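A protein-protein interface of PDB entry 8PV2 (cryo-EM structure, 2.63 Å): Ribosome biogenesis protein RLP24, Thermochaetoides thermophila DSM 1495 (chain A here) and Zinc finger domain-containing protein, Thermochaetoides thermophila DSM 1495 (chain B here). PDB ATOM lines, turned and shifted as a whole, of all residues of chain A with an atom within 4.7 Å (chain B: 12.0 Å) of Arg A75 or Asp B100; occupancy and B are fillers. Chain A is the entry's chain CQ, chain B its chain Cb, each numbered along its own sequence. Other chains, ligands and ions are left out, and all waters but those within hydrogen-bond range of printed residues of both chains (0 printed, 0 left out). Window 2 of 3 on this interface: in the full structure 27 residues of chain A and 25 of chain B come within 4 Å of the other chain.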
ATOM      1  N   PHE A  71      -9.057   0.645 -17.755  1.00  0.00           N
ATOM      2  CA  PHE A  71      -8.424   0.361 -19.034  1.00  0.00           C
ATOM      3  C   PHE A  71      -6.957   0.761 -19.096  1.00  0.00           C
ATOM      4  O   PHE A  71      -6.235   0.262 -19.964  1.00  0.00           O
ATOM      5  CB  PHE A  71      -9.182   1.058 -20.162  1.00  0.00           C
ATOM      6  CG  PHE A  71     -10.550   0.499 -20.409  1.00  0.00           C
ATOM      7  CD1 PHE A  71     -10.738  -0.530 -21.314  1.00  0.00           C
ATOM      8  CD2 PHE A  71     -11.653   1.011 -19.749  1.00  0.00           C
ATOM      9  CE1 PHE A  71     -11.995  -1.041 -21.552  1.00  0.00           C
ATOM     10  CE2 PHE A  71     -12.913   0.502 -19.982  1.00  0.00           C
ATOM     11  CZ  PHE A  71     -13.083  -0.525 -20.883  1.00  0.00           C
ATOM     12  N   ALA A  72      -6.497   1.636 -18.210  1.00  0.00           N
ATOM     13  CA  ALA A  72      -5.106   2.066 -18.183  1.00  0.00           C
ATOM     14  C   ALA A  72      -4.393   1.402 -17.016  1.00  0.00           C
ATOM     15  O   ALA A  72      -4.845   1.496 -15.872  1.00  0.00           O
ATOM     16  CB  ALA A  72      -4.999   3.586 -18.073  1.00  0.00           C
ATOM     17  N   ALA A  73      -3.278   0.737 -17.311  1.00  0.00           N
ATOM     18  CA  ALA A  73      -2.518   0.026 -16.298  1.00  0.00           C
ATOM     19  C   ALA A  73      -1.064  -0.049 -16.730  1.00  0.00           C
ATOM     20  O   ALA A  73      -0.737   0.109 -17.907  1.00  0.00           O
ATOM     21  CB  ALA A  73      -3.070  -1.382 -16.062  1.00  0.00           C
ATOM     22  N   ARG A  74      -0.190  -0.291 -15.758  1.00  0.00           N
ATOM     23  CA  ARG A  74       1.215  -0.554 -16.043  1.00  0.00           C
ATOM     24  C   ARG A  74       1.343  -2.001 -16.497  1.00  0.00           C
ATOM     25  O   ARG A  74       1.321  -2.921 -15.673  1.00  0.00           O
ATOM     26  CB  ARG A  74       2.072  -0.275 -14.811  1.00  0.00           C
ATOM     27  CG  ARG A  74       3.566  -0.456 -15.029  1.00  0.00           C
ATOM     28  CD  ARG A  74       4.339  -0.180 -13.755  1.00  0.00           C
ATOM     29  NE  ARG A  74       5.636   0.426 -14.031  1.00  0.00           N
ATOM     30  CZ  ARG A  74       6.788  -0.227 -14.041  1.00  0.00           C
ATOM     31  NH1 ARG A  74       6.857  -1.511 -13.746  1.00  0.00           N
ATOM     32  NH2 ARG A  74       7.902   0.430 -14.349  1.00  0.00           N
ATOM     33  N   ARG A  75       1.471  -2.209 -17.803  1.00  0.00           N
ATOM     34  CA  ARG A  75       1.485  -3.548 -18.381  1.00  0.00           C
ATOM     35  C   ARG A  75       2.883  -4.133 -18.241  1.00  0.00           C
ATOM     36  O   ARG A  75       3.802  -3.749 -18.970  1.00  0.00           O
ATOM     37  CB  ARG A  75       1.052  -3.513 -19.841  1.00  0.00           C
ATOM     38  CG  ARG A  75      -0.152  -2.644 -20.100  1.00  0.00           C
ATOM     39  CD  ARG A  75      -1.419  -3.274 -19.572  1.00  0.00           C
ATOM     40  NE  ARG A  75      -2.576  -2.433 -19.845  1.00  0.00           N
ATOM     41  CZ  ARG A  75      -3.829  -2.783 -19.605  1.00  0.00           C
ATOM     42  NH1 ARG A  75      -4.128  -3.956 -19.074  1.00  0.00           N
ATOM     43  NH2 ARG A  75      -4.808  -1.935 -19.901  1.00  0.00           N
ATOM     44  N   ASN A  76       3.038  -5.073 -17.315  1.00  0.00           N
ATOM     45  CA  ASN A  76       4.319  -5.709 -17.061  1.00  0.00           C
ATOM     46  C   ASN A  76       4.524  -6.987 -17.859  1.00  0.00           C
ATOM     47  O   ASN A  76       5.588  -7.603 -17.750  1.00  0.00           O
ATOM     48  CB  ASN A  76       4.462  -6.004 -15.570  1.00  0.00           C
ATOM     49  CG  ASN A  76       4.826  -4.775 -14.776  1.00  0.00           C
ATOM     50  OD1 ASN A  76       5.281  -3.781 -15.331  1.00  0.00           O
ATOM     51  ND2 ASN A  76       4.630  -4.836 -13.469  1.00  0.00           N
ATOM     52  N   VAL A  77       3.535  -7.405 -18.640  1.00  0.00           N
ATOM     53  CA  VAL A  77       3.683  -8.515 -19.576  1.00  0.00           C
ATOM     54  C   VAL A  77       3.525  -7.959 -20.984  1.00  0.00           C
ATOM     55  O   VAL A  77       2.412  -7.585 -21.373  1.00  0.00           O
ATOM     56  CB  VAL A  77       2.668  -9.630 -19.296  1.00  0.00           C
ATOM     57  CG1 VAL A  77       2.831 -10.744 -20.301  1.00  0.00           C
ATOM     58  CG2 VAL A  77       2.850 -10.158 -17.892  1.00  0.00           C
ATOM     59  N   MET B  92      -0.461   6.332  -6.861  1.00  0.00           N
ATOM     60  CA  MET B  92      -1.021   5.695  -8.044  1.00  0.00           C
ATOM     61  C   MET B  92      -2.546   5.627  -7.966  1.00  0.00           C
ATOM     62  O   MET B  92      -3.247   5.871  -8.960  1.00  0.00           O
ATOM     63  CB  MET B  92      -0.393   4.311  -8.178  1.00  0.00           C
ATOM     64  CG  MET B  92      -0.752   3.548  -9.403  1.00  0.00           C
ATOM     65  SD  MET B  92       0.054   1.944  -9.463  1.00  0.00           S
ATOM     66  CE  MET B  92       1.734   2.446  -9.802  1.00  0.00           C
ATOM     67  N   GLY B  96      -5.826   6.932 -10.109  1.00  0.00           N
ATOM     68  CA  GLY B  96      -6.628   5.831 -10.604  1.00  0.00           C
ATOM     69  C   GLY B  96      -5.860   4.925 -11.528  1.00  0.00           C
ATOM     70  O   GLY B  96      -6.450   4.269 -12.390  1.00  0.00           O
ATOM     71  N   TYR B  97      -4.548   4.885 -11.370  1.00  0.00           N
ATOM     72  CA  TYR B  97      -3.655   4.080 -12.176  1.00  0.00           C
ATOM     73  C   TYR B  97      -3.424   2.777 -11.424  1.00  0.00           C
ATOM     74  O   TYR B  97      -3.726   2.679 -10.232  1.00  0.00           O
ATOM     75  CB  TYR B  97      -2.358   4.859 -12.413  1.00  0.00           C
ATOM     76  CG  TYR B  97      -1.356   4.269 -13.367  1.00  0.00           C
ATOM     77  CD1 TYR B  97      -1.694   4.016 -14.686  1.00  0.00           C
ATOM     78  CD2 TYR B  97      -0.052   4.028 -12.965  1.00  0.00           C
ATOM     79  CE1 TYR B  97      -0.773   3.504 -15.565  1.00  0.00           C
ATOM     80  CE2 TYR B  97       0.876   3.517 -13.837  1.00  0.00           C
ATOM     81  CZ  TYR B  97       0.510   3.256 -15.136  1.00  0.00           C
ATOM     82  OH  TYR B  97       1.432   2.744 -16.015  1.00  0.00           O
ATOM     83  N   ARG B  98      -2.929   1.761 -12.121  1.00  0.00           N
ATOM     84  CA  ARG B  98      -2.745   0.452 -11.510  1.00  0.00           C
ATOM     85  C   ARG B  98      -1.680  -0.323 -12.270  1.00  0.00           C
ATOM     86  O   ARG B  98      -1.161   0.128 -13.293  1.00  0.00           O
ATOM     87  CB  ARG B  98      -4.067  -0.320 -11.455  1.00  0.00           C
ATOM     88  CG  ARG B  98      -4.636  -0.645 -12.807  1.00  0.00           C
ATOM     89  CD  ARG B  98      -5.947  -1.383 -12.702  1.00  0.00           C
ATOM     90  NE  ARG B  98      -6.488  -1.678 -14.022  1.00  0.00           N
ATOM     91  CZ  ARG B  98      -6.249  -2.794 -14.695  1.00  0.00           C
ATOM     92  NH1 ARG B  98      -5.501  -3.760 -14.190  1.00  0.00           N
ATOM     93  NH2 ARG B  98      -6.773  -2.943 -15.908  1.00  0.00           N
ATOM     94  N   ILE B  99      -1.343  -1.497 -11.747  1.00  0.00           N
ATOM     95  CA  ILE B  99      -0.301  -2.350 -12.306  1.00  0.00           C
ATOM     96  C   ILE B  99      -0.937  -3.667 -12.723  1.00  0.00           C
ATOM     97  O   ILE B  99      -1.631  -4.311 -11.926  1.00  0.00           O
ATOM     98  CB  ILE B  99       0.840  -2.579 -11.304  1.00  0.00           C
ATOM     99  CG1 ILE B  99       1.449  -1.246 -10.875  1.00  0.00           C
ATOM    100  CG2 ILE B  99       1.912  -3.452 -11.909  1.00  0.00           C
ATOM    101  CD1 ILE B  99       2.281  -1.337  -9.624  1.00  0.00           C
ATOM    102  N   ASP B 100      -0.704  -4.065 -13.969  1.00  0.00           N
ATOM    103  CA  ASP B 100      -1.176  -5.337 -14.498  1.00  0.00           C
ATOM    104  C   ASP B 100       0.017  -6.283 -14.574  1.00  0.00           C
ATOM    105  O   ASP B 100       0.887  -6.120 -15.434  1.00  0.00           O
ATOM    106  CB  ASP B 100      -1.820  -5.141 -15.872  1.00  0.00           C
ATOM    107  CG  ASP B 100      -2.488  -6.401 -16.407  1.00  0.00           C
ATOM    108  OD1 ASP B 100      -3.717  -6.366 -16.627  1.00  0.00           O
ATOM    109  OD2 ASP B 100      -1.800  -7.415 -16.648  1.00  0.00           O
ATOM    110  N   ASN B 101       0.049  -7.269 -13.680  1.00  0.00           N
ATOM    111  CA  ASN B 101       1.144  -8.227 -13.601  1.00  0.00           C
ATOM    112  C   ASN B 101       0.767  -9.586 -14.177  1.00  0.00           C
ATOM    113  O   ASN B 101       1.454 -10.577 -13.915  1.00  0.00           O
ATOM    114  CB  ASN B 101       1.605  -8.379 -12.153  1.00  0.00           C
ATOM    115  CG  ASN B 101       2.517  -7.260 -11.719  1.00  0.00           C
ATOM    116  OD1 ASN B 101       3.039  -6.519 -12.547  1.00  0.00           O
ATOM    117  ND2 ASN B 101       2.713  -7.126 -10.415  1.00  0.00           N
ATOM    118  N   GLY B 102      -0.313  -9.654 -14.946  1.00  0.00           N
ATOM    119  CA  GLY B 102      -0.767 -10.910 -15.506  1.00  0.00           C
ATOM    120  C   GLY B 102      -1.959 -11.485 -14.770  1.00  0.00           C
ATOM    121  O   GLY B 102      -2.931 -11.919 -15.388  1.00  0.00           O
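The side-chain amide nitrogen (ND2) of Asn A76 lies within hydrogen-bond range of the side-chain amide oxygen (OD1) of Asn B101. OH of Tyr B97 sits close to N of Arg A74 (3.5 Å). The backbone NH (N) of Asn A76 lies within hydrogen-bond range of the backbone carbonyl oxygen (O) of Asp B100. NH1 of Arg A75 is in salt-bridge range of OD1 of Asp B100 (3.5 Å). O of Arg A74 is in hydrogen-bond range of N of Asp B100, 2.9 Å away. The backbone NH (N) of Arg A74 sits at hydrogen-bond distance from the backbone carbonyl oxygen (O) of Arg B98 (2.7 Å).
O of Met B92 sits at hydrogen-bond distance from N of Tyr B97 (2.9 Å). The backbone carbonyl oxygen (O) of Phe A71 lies within hydrogen-bond range of the guanidinium group (NH2) of Arg A75 (2.6 Å). The guanidinium group of Arg A74 is in hydrogen-bond range of the side-chain amide oxygen of Asn A76 (3.2 Å). The guanidinium group (NH1) of Arg B98 is in salt-bridge range of the side-chain carboxylate (OD1) of Asp B100 (3.99 Å). The backbone NH (N) of Gly B102 is in hydrogen-bond range of the side-chain carboxylate (OD2) of Asp B100 (3.2 Å).
O of Ala A72 touches CG of Arg B98 (3.7 Å). Ala A73 touches Tyr B97. Arg B98 touches Ala A73 (O to CA, 3.3 Å). Ala A73 touches Asp B100 (CB to CB, 3.97 Å). Arg A74 touches Ile B99 (O to CA, 3.8 Å). Ile B99 touches Asn A76.
Arg A75 touches one residue of chain B. Asp B100 touches four residues of chain A. Of chain B, only Arg B98 (3.7 Å) comes within 4 Å of Ala A72. Arg A74 touches four residues of chain B. Asn A76 touches just these residues of chain B: Ile B99, Asp B100 and Asn B101. No residue of chain B comes within 4 Å of Val A77. Of the printed residues of chain A, Arg B98 touches Ala A72, Ala A73 and Arg A74. Printed residues of chain A within 4 Å of Ile B99: Arg A74 and Asn A76. Of the printed residues of chain A, Asn B101 touches Asn A76. Gly B96 touches none of the printed residues of chain A. Gly B102 touches none of the printed residues of chain A. The nearest residue of chain B that does not touch Arg A75 is Arg B98 (4.2 Å). The nearest residue of chain A that does not touch Asp B100 is Val A77 (4.4 Å).
Of the 7 printed residues of chain A, 5 touch a printed residue of chain B. Printed residues of chain A that touch a printed residue of chain B: Ala A72, Ala A73, Arg A74, Arg A75 and Asn A76. Hydrophobic or aromatic side chains of chain A that line the printed part of chain B: Ala A73. Printed residues of chain B that touch a printed residue of chain A: Tyr B97, Arg B98, Ile B99, Asp B100 and Asn B101. Along chain B the printed residues that touch a printed residue of chain A span positions 97 to 101. Among the printed residues, 12 pairs touch across the chains. Among the printed residues, Asp or Glu carboxylates within 4 Å of a Lys or Arg side-chain nitrogen of the other chain: Arg A75 with Asp B100.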
